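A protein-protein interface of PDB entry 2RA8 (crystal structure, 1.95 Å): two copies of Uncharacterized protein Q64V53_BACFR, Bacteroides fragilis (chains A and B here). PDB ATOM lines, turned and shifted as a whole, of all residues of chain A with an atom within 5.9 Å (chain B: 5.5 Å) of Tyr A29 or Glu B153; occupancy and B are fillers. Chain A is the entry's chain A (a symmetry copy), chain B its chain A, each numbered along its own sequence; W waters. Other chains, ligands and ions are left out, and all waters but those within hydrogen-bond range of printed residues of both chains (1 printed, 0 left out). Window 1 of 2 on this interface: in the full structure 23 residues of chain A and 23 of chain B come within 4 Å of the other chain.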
ATOM      1  N   PHE A  15      28.685  18.804  30.586  1.00  0.00           N
ATOM      2  CA  PHE A  15      28.984  20.219  30.397  1.00  0.00           C
ATOM      3  C   PHE A  15      27.713  20.987  30.164  1.00  0.00           C
ATOM      4  O   PHE A  15      26.685  20.432  29.750  1.00  0.00           O
ATOM      5  CB  PHE A  15      29.913  20.456  29.186  1.00  0.00           C
ATOM      6  CG  PHE A  15      29.242  20.240  27.855  1.00  0.00           C
ATOM      7  CD1 PHE A  15      29.042  18.954  27.362  1.00  0.00           C
ATOM      8  CD2 PHE A  15      28.769  21.319  27.116  1.00  0.00           C
ATOM      9  CE1 PHE A  15      28.373  18.748  26.157  1.00  0.00           C
ATOM     10  CE2 PHE A  15      28.099  21.117  25.907  1.00  0.00           C
ATOM     11  CZ  PHE A  15      27.902  19.828  25.432  1.00  0.00           C
ATOM     12  N   TRP A  16      27.797  22.287  30.414  1.00  0.00           N
ATOM     13  CA  TRP A  16      26.680  23.198  30.244  1.00  0.00           C
ATOM     14  C   TRP A  16      27.304  24.507  29.839  1.00  0.00           C
ATOM     15  O   TRP A  16      28.211  24.996  30.515  1.00  0.00           O
ATOM     16  CB  TRP A  16      25.926  23.347  31.578  1.00  0.00           C
ATOM     17  CG  TRP A  16      24.757  24.295  31.559  1.00  0.00           C
ATOM     18  CD1 TRP A  16      23.465  24.008  31.207  1.00  0.00           C
ATOM     19  CD2 TRP A  16      24.780  25.681  31.923  1.00  0.00           C
ATOM     20  NE1 TRP A  16      22.678  25.133  31.333  1.00  0.00           N
ATOM     21  CE2 TRP A  16      23.456  26.170  31.769  1.00  0.00           C
ATOM     22  CE3 TRP A  16      25.784  26.551  32.369  1.00  0.00           C
ATOM     23  CZ2 TRP A  16      23.117  27.500  32.044  1.00  0.00           C
ATOM     24  CZ3 TRP A  16      25.445  27.880  32.645  1.00  0.00           C
ATOM     25  CH2 TRP A  16      24.115  28.338  32.480  1.00  0.00           C
ATOM     26  N   SER A  17      26.866  25.065  28.715  1.00  0.00           N
ATOM     27  CA  SER A  17      27.405  26.343  28.262  1.00  0.00           C
ATOM     28  C   SER A  17      26.286  27.312  28.006  1.00  0.00           C
ATOM     29  O   SER A  17      25.162  26.916  27.664  1.00  0.00           O
ATOM     30  CB  SER A  17      28.262  26.175  26.993  1.00  0.00           C
ATOM     31  OG  SER A  17      27.483  25.913  25.840  1.00  0.00           O
ATOM     32  N   VAL A  27      21.640  28.044  25.383  1.00  0.00           N
ATOM     33  CA  VAL A  27      22.201  27.022  26.259  1.00  0.00           C
ATOM     34  C   VAL A  27      22.507  25.772  25.465  1.00  0.00           C
ATOM     35  O   VAL A  27      21.733  25.364  24.585  1.00  0.00           O
ATOM     36  CB  VAL A  27      21.201  26.664  27.400  1.00  0.00           C
ATOM     37  CG1 VAL A  27      21.585  25.352  28.051  1.00  0.00           C
ATOM     38  CG2 VAL A  27      21.180  27.772  28.447  1.00  0.00           C
ATOM     39  N   ASN A  28      23.646  25.165  25.777  1.00  0.00           N
ATOM     40  CA  ASN A  28      24.101  23.939  25.133  1.00  0.00           C
ATOM     41  C   ASN A  28      24.537  23.023  26.258  1.00  0.00           C
ATOM     42  O   ASN A  28      25.405  23.387  27.059  1.00  0.00           O
ATOM     43  CB  ASN A  28      25.284  24.252  24.207  1.00  0.00           C
ATOM     44  CG  ASN A  28      25.809  23.024  23.481  1.00  0.00           C
ATOM     45  OD1 ASN A  28      26.984  22.968  23.108  1.00  0.00           O
ATOM     46  ND2 ASN A  28      24.943  22.045  23.259  1.00  0.00           N
ATOM     47  N   TYR A  29      23.940  21.835  26.334  1.00  0.00           N
ATOM     48  CA  TYR A  29      24.272  20.886  27.391  1.00  0.00           C
ATOM     49  C   TYR A  29      24.272  19.454  26.960  1.00  0.00           C
ATOM     50  O   TYR A  29      23.508  19.063  26.080  1.00  0.00           O
ATOM     51  CB  TYR A  29      23.295  21.023  28.565  1.00  0.00           C
ATOM     52  CG  TYR A  29      21.874  20.602  28.250  1.00  0.00           C
ATOM     53  CD1 TYR A  29      21.038  21.408  27.481  1.00  0.00           C
ATOM     54  CD2 TYR A  29      21.374  19.384  28.709  1.00  0.00           C
ATOM     55  CE1 TYR A  29      19.731  21.008  27.174  1.00  0.00           C
ATOM     56  CE2 TYR A  29      20.072  18.973  28.410  1.00  0.00           C
ATOM     57  CZ  TYR A  29      19.261  19.790  27.643  1.00  0.00           C
ATOM     58  OH  TYR A  29      17.978  19.386  27.347  1.00  0.00           O
ATOM     59  N   GLY A  30      25.111  18.650  27.607  1.00  0.00           N
ATOM     60  CA  GLY A  30      25.188  17.238  27.277  1.00  0.00           C
ATOM     61  C   GLY A  30      26.335  16.534  27.978  1.00  0.00           C
ATOM     62  O   GLY A  30      27.021  17.122  28.822  1.00  0.00           O
ATOM     63  N   LYS A  31      26.538  15.267  27.632  1.00  0.00           N
ATOM     64  CA  LYS A  31      27.606  14.466  28.209  1.00  0.00           C
ATOM     65  C   LYS A  31      28.916  14.931  27.629  1.00  0.00           C
ATOM     66  O   LYS A  31      28.987  15.291  26.448  1.00  0.00           O
ATOM     67  CB  LYS A  31      27.384  12.983  27.871  1.00  0.00           C
ATOM     68  CG  LYS A  31      28.372  12.015  28.510  1.00  0.00           C
ATOM     69  CD  LYS A  31      28.102  10.572  28.092  1.00  0.00           C
ATOM     70  CE  LYS A  31      26.763  10.066  28.606  1.00  0.00           C
ATOM     71  NZ  LYS A  31      26.497   8.673  28.154  1.00  0.00           N
ATOM     72  N   ASP A  35      28.132  16.616  21.288  1.00  0.00           N
ATOM     73  CA  ASP A  35      27.645  17.942  20.923  1.00  0.00           C
ATOM     74  C   ASP A  35      26.553  18.364  21.870  1.00  0.00           C
ATOM     75  O   ASP A  35      26.327  19.556  22.075  1.00  0.00           O
ATOM     76  CB  ASP A  35      27.085  17.960  19.490  1.00  0.00           C
ATOM     77  CG  ASP A  35      28.092  17.484  18.459  1.00  0.00           C
ATOM     78  OD1 ASP A  35      29.283  17.853  18.572  1.00  0.00           O
ATOM     79  OD2 ASP A  35      27.687  16.749  17.528  1.00  0.00           O
ATOM     80  N   GLY A  36      25.861  17.389  22.448  1.00  0.00           N
ATOM     81  CA  GLY A  36      24.786  17.706  23.370  1.00  0.00           C
ATOM     82  C   GLY A  36      23.575  18.325  22.689  1.00  0.00           C
ATOM     83  O   GLY A  36      23.424  18.232  21.470  1.00  0.00           O
ATOM     84  N   GLN A  37      22.714  18.956  23.481  1.00  0.00           N
ATOM     85  CA  GLN A  37      21.496  19.585  22.971  1.00  0.00           C
ATOM     86  C   GLN A  37      21.578  21.082  23.090  1.00  0.00           C
ATOM     87  O   GLN A  37      22.453  21.613  23.774  1.00  0.00           O
ATOM     88  CB  GLN A  37      20.286  19.100  23.768  1.00  0.00           C
ATOM     89  CG  GLN A  37      20.207  17.588  23.923  1.00  0.00           C
ATOM     90  CD  GLN A  37      19.216  17.166  24.990  1.00  0.00           C
ATOM     91  OE1 GLN A  37      19.572  16.470  25.938  1.00  0.00           O
ATOM     92  NE2 GLN A  37      17.966  17.585  24.842  1.00  0.00           N
ATOM     93  N   THR A  38      20.657  21.775  22.430  1.00  0.00           N
ATOM     94  CA  THR A  38      20.633  23.230  22.473  1.00  0.00           C
ATOM     95  C   THR A  38      19.258  23.769  22.712  1.00  0.00           C
ATOM     96  O   THR A  38      18.286  23.322  22.107  1.00  0.00           O
ATOM     97  CB  THR A  38      21.187  23.833  21.169  1.00  0.00           C
ATOM     98  OG1 THR A  38      22.580  23.518  21.059  1.00  0.00           O
ATOM     99  CG2 THR A  38      21.007  25.348  21.158  1.00  0.00           C
ATOM    100  N   GLN A  39      19.176  24.741  23.613  1.00  0.00           N
ATOM    101  CA  GLN A  39      17.922  25.383  23.955  1.00  0.00           C
ATOM    102  C   GLN A  39      18.113  26.865  23.786  1.00  0.00           C
ATOM    103  O   GLN A  39      19.115  27.430  24.236  1.00  0.00           O
ATOM    104  CB  GLN A  39      17.530  25.068  25.402  1.00  0.00           C
ATOM    105  CG  GLN A  39      17.425  23.580  25.704  1.00  0.00           C
ATOM    106  CD  GLN A  39      17.029  23.296  27.140  1.00  0.00           C
ATOM    107  OE1 GLN A  39      17.588  23.871  28.073  1.00  0.00           O
ATOM    108  NE2 GLN A  39      16.067  22.395  27.327  1.00  0.00           N
ATOM    109  N   LYS B  82       8.422   0.780  28.002  1.00  0.00           N
ATOM    110  CA  LYS B  82       8.808   2.144  27.680  1.00  0.00           C
ATOM    111  C   LYS B  82       9.747   2.129  26.496  1.00  0.00           C
ATOM    112  O   LYS B  82      10.714   1.371  26.474  1.00  0.00           O
ATOM    113  CB  LYS B  82       9.518   2.785  28.875  1.00  0.00           C
ATOM    114  CG  LYS B  82      10.031   4.191  28.615  1.00  0.00           C
ATOM    115  CD  LYS B  82      10.645   4.772  29.874  1.00  0.00           C
ATOM    116  CE  LYS B  82      11.179   6.183  29.649  1.00  0.00           C
ATOM    117  NZ  LYS B  82      11.606   6.760  30.946  1.00  0.00           N
ATOM    118  N   LEU B  85      14.619   6.713  22.915  1.00  0.00           N
ATOM    119  CA  LEU B  85      15.835   6.788  22.116  1.00  0.00           C
ATOM    120  C   LEU B  85      16.935   7.377  22.946  1.00  0.00           C
ATOM    121  O   LEU B  85      16.755   8.420  23.571  1.00  0.00           O
ATOM    122  CB  LEU B  85      15.649   7.689  20.884  1.00  0.00           C
ATOM    123  CG  LEU B  85      15.182   7.112  19.541  1.00  0.00           C
ATOM    124  CD1 LEU B  85      15.104   8.240  18.519  1.00  0.00           C
ATOM    125  CD2 LEU B  85      16.146   6.039  19.057  1.00  0.00           C
ATOM    126  N   CAS B 116      11.958   9.789  25.394  1.00  0.00           N
ATOM    127  CA  CAS B 116      12.601  10.835  24.578  1.00  0.00           C
ATOM    128  CB  CAS B 116      14.061  10.807  25.093  1.00  0.00           C
ATOM    129  C   CAS B 116      12.605  10.439  23.088  1.00  0.00           C
ATOM    130  O   CAS B 116      13.043   9.339  22.728  1.00  0.00           O
ATOM    131  SG  CAS B 116      14.864  12.094  24.192  1.00  0.00           S
ATOM    132 AS   CAS B 116      14.084  14.021  25.146  1.00  0.00          AS
ATOM    133  CE1 CAS B 116      15.787  14.971  25.706  1.00  0.00           C
ATOM    134  CE2 CAS B 116      12.775  14.857  23.966  1.00  0.00           C
ATOM    135  N   TYR B 119      17.014  14.540  19.816  1.00  0.00           N
ATOM    136  CA  TYR B 119      17.900  15.471  20.495  1.00  0.00           C
ATOM    137  C   TYR B 119      18.214  16.672  19.641  1.00  0.00           C
ATOM    138  O   TYR B 119      19.201  17.366  19.874  1.00  0.00           O
ATOM    139  CB  TYR B 119      19.196  14.750  20.892  1.00  0.00           C
ATOM    140  CG  TYR B 119      18.983  13.636  21.891  1.00  0.00           C
ATOM    141  CD1 TYR B 119      19.020  13.885  23.259  1.00  0.00           C
ATOM    142  CD2 TYR B 119      18.690  12.345  21.465  1.00  0.00           C
ATOM    143  CE1 TYR B 119      18.768  12.872  24.182  1.00  0.00           C
ATOM    144  CE2 TYR B 119      18.435  11.326  22.377  1.00  0.00           C
ATOM    145  CZ  TYR B 119      18.475  11.599  23.729  1.00  0.00           C
ATOM    146  OH  TYR B 119      18.202  10.600  24.628  1.00  0.00           O
ATOM    147  N   ASP B 148       7.295  10.621  28.825  1.00  0.00           N
ATOM    148  CA  ASP B 148       8.010  10.282  30.045  1.00  0.00           C
ATOM    149  C   ASP B 148       9.455  10.699  29.889  1.00  0.00           C
ATOM    150  O   ASP B 148      10.350   9.869  29.704  1.00  0.00           O
ATOM    151  CB  ASP B 148       7.890   8.790  30.324  1.00  0.00           C
ATOM    152  CG  ASP B 148       8.500   8.388  31.658  1.00  0.00           C
ATOM    153  OD1 ASP B 148       8.584   9.241  32.562  1.00  0.00           O
ATOM    154  OD2 ASP B 148       8.876   7.208  31.807  1.00  0.00           O
ATOM    155  N   ILE B 149       9.651  12.014  29.961  1.00  0.00           N
ATOM    156  CA  ILE B 149      10.948  12.675  29.820  1.00  0.00           C
ATOM    157  C   ILE B 149      11.378  13.239  31.156  1.00  0.00           C
ATOM    158  O   ILE B 149      10.726  14.139  31.689  1.00  0.00           O
ATOM    159  CB  ILE B 149      10.853  13.875  28.848  1.00  0.00           C
ATOM    160  CG1 ILE B 149      10.034  13.500  27.612  1.00  0.00           C
ATOM    161  CG2 ILE B 149      12.255  14.382  28.515  1.00  0.00           C
ATOM    162  CD1 ILE B 149      10.534  12.306  26.872  1.00  0.00           C
ATOM    163  N   ASP B 150      12.487  12.741  31.688  1.00  0.00           N
ATOM    164  CA  ASP B 150      12.998  13.203  32.976  1.00  0.00           C
ATOM    165  C   ASP B 150      13.696  14.539  32.928  1.00  0.00           C
ATOM    166  O   ASP B 150      14.140  14.990  31.872  1.00  0.00           O
ATOM    167  CB  ASP B 150      13.952  12.160  33.568  1.00  0.00           C
ATOM    168  CG  ASP B 150      13.219  11.008  34.235  1.00  0.00           C
ATOM    169  OD1 ASP B 150      12.328  10.409  33.596  1.00  0.00           O
ATOM    170  OD2 ASP B 150      13.538  10.701  35.403  1.00  0.00           O
ATOM    171  N   PHE B 151      13.800  15.166  34.097  1.00  0.00           N
ATOM    172  CA  PHE B 151      14.438  16.473  34.259  1.00  0.00           C
ATOM    173  C   PHE B 151      15.796  16.549  33.594  1.00  0.00           C
ATOM    174  O   PHE B 151      16.081  17.510  32.886  1.00  0.00           O
ATOM    175  CB  PHE B 151      14.592  16.790  35.755  1.00  0.00           C
ATOM    176  CG  PHE B 151      14.957  18.216  36.047  1.00  0.00           C
ATOM    177  CD1 PHE B 151      14.005  19.226  35.957  1.00  0.00           C
ATOM    178  CD2 PHE B 151      16.248  18.548  36.440  1.00  0.00           C
ATOM    179  CE1 PHE B 151      14.339  20.539  36.256  1.00  0.00           C
ATOM    180  CE2 PHE B 151      16.583  19.863  36.740  1.00  0.00           C
ATOM    181  CZ  PHE B 151      15.628  20.854  36.648  1.00  0.00           C
ATOM    182  N   GLU B 152      16.632  15.535  33.821  1.00  0.00           N
ATOM    183  CA  GLU B 152      17.984  15.484  33.253  1.00  0.00           C
ATOM    184  C   GLU B 152      18.036  15.473  31.751  1.00  0.00           C
ATOM    185  O   GLU B 152      18.969  16.009  31.143  1.00  0.00           O
ATOM    186  CB  GLU B 152      18.731  14.252  33.749  1.00  0.00           C
ATOM    187  CG  GLU B 152      19.611  14.485  34.955  1.00  0.00           C
ATOM    188  CD  GLU B 152      20.633  13.380  35.122  1.00  0.00           C
ATOM    189  OE1 GLU B 152      20.225  12.210  35.284  1.00  0.00           O
ATOM    190  OE2 GLU B 152      21.846  13.677  35.084  1.00  0.00           O
ATOM    191  N   GLU B 153      17.048  14.834  31.137  1.00  0.00           N
ATOM    192  CA  GLU B 153      16.984  14.756  29.687  1.00  0.00           C
ATOM    193  C   GLU B 153      16.637  16.122  29.143  1.00  0.00           C
ATOM    194  O   GLU B 153      17.279  16.618  28.214  1.00  0.00           O
ATOM    195  CB  GLU B 153      15.942  13.705  29.277  1.00  0.00           C
ATOM    196  CG  GLU B 153      16.296  12.287  29.763  1.00  0.00           C
ATOM    197  CD  GLU B 153      15.248  11.247  29.397  1.00  0.00           C
ATOM    198  OE1 GLU B 153      14.162  11.247  30.009  1.00  0.00           O
ATOM    199  OE2 GLU B 153      15.512  10.427  28.496  1.00  0.00           O
ATOM    200  N   GLN B 154      15.617  16.738  29.734  1.00  0.00           N
ATOM    201  CA  GLN B 154      15.176  18.072  29.360  1.00  0.00           C
ATOM    202  C   GLN B 154      14.021  18.456  30.275  1.00  0.00           C
ATOM    203  O   GLN B 154      13.137  17.645  30.555  1.00  0.00           O
ATOM    204  CB  GLN B 154      14.782  18.113  27.858  1.00  0.00           C
ATOM    205  CG  GLN B 154      13.313  18.327  27.548  1.00  0.00           C
ATOM    206  CD  GLN B 154      12.992  18.184  26.062  1.00  0.00           C
ATOM    207  OE1 GLN B 154      11.926  17.676  25.694  1.00  0.00           O
ATOM    208  NE2 GLN B 154      13.901  18.643  25.204  1.00  0.00           N
ATOM    209  N   GLU B 155      14.040  19.689  30.769  1.00  0.00           N
ATOM    210  CA  GLU B 155      12.997  20.169  31.669  1.00  0.00           C
ATOM    211  C   GLU B 155      11.631  20.106  31.043  1.00  0.00           C
ATOM    212  O   GLU B 155      11.474  20.270  29.837  1.00  0.00           O
ATOM    213  CB  GLU B 155      13.273  21.602  32.111  1.00  0.00           C
ATOM    214  CG  GLU B 155      14.485  21.762  33.009  1.00  0.00           C
ATOM    215  CD  GLU B 155      14.439  23.065  33.780  1.00  0.00           C
ATOM    216  OE1 GLU B 155      15.266  23.960  33.508  1.00  0.00           O
ATOM    217  OE2 GLU B 155      13.559  23.192  34.659  1.00  0.00           O
HETATM  218  O   HOH W   1      19.028  19.998  20.968  1.00  0.00           O
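The backbone NH (N) of Leu B85 lies within hydrogen-bond range of O of CAS B116, 3.1 Å away. The side-chain hydroxyl (OH) of Tyr B119 sits close to SG of CAS B116 (3.7 Å). The side-chain hydroxyl (OH) of Tyr B119 is in hydrogen-bond range of the backbone carbonyl oxygen (O) of Leu B85, at 2.8 Å. The backbone NH of Asp B150 sits at hydrogen-bond distance from the side-chain carboxylate of Glu B153 (2.8 Å). O of Tyr A29 sits at hydrogen-bond distance from N of Gln A37, at 2.7 Å. The side-chain amide nitrogen (ND2) of Asn A28 lies within hydrogen-bond range of the backbone carbonyl oxygen (O) of Gln A37 (2.6 Å).
Tyr A29 touches Gln B154. Gln A37 touches CAS B116. Gln A37 touches Tyr B119 (CD to CD1, 3.7 Å).
Tyr A29 touches just these residues of chain B: Glu B153 and Gln B154. Lys A31 touches none of the printed residues of chain B. Printed residues of chain B within 4 Å of Gln A37: CAS B116 (3.5 Å), Tyr B119 (3.7 Å) and Glu B153 (3.2 Å). Printed residues of chain A within 4 Å of Tyr B119: Gln A37 (3.7 Å). Asp B150 touches none of the printed residues of chain A. Glu B153 touches just these residues of chain A: Tyr A29 and Gln A37. Printed residues of chain A within 4 Å of Gln B154: Tyr A29 (3.5 Å). The nearest printed residue of chain A that does not touch Glu B153 is Gln A39 (6.0 Å). The nearest printed residue of chain A that does not touch Gln B154 is Gln A37 (4.2 Å).
No position is printed for both chains. Of the 5 pairs that touch across the chains among the printed residues, none has its exchanged pair printed and touching as well.
Water W1 lies within hydrogen-bond range of the backbone NH of Thr A38 (2.8 Å) and the backbone carbonyl oxygen of Tyr B119 (2.9 Å).
The backbone carbonyl oxygen of Glu B153 sits close to the side-chain amide oxygen of Gln A37, 3.2 Å away. The backbone carbonyl oxygen (O) of Glu B153 lies within hydrogen-bond range of the side-chain hydroxyl (OH) of Tyr A29 (3.0 Å).
Printed residues of chain B that touch a printed residue of chain A: CAS B116, Tyr B119, Glu B153 and Gln B154. Of the 13 printed residues of chain A, 2 touch a printed residue of chain B. Hydrophobic or aromatic side chains of chain A within 4 Å of the printed part of chain B: Tyr A29. Among the printed residues, 5 pairs touch across the chains. Among the printed residues, no Asp or Glu carboxylate lies within 4 Å of a Lys or Arg side-chain nitrogen of the other chain.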
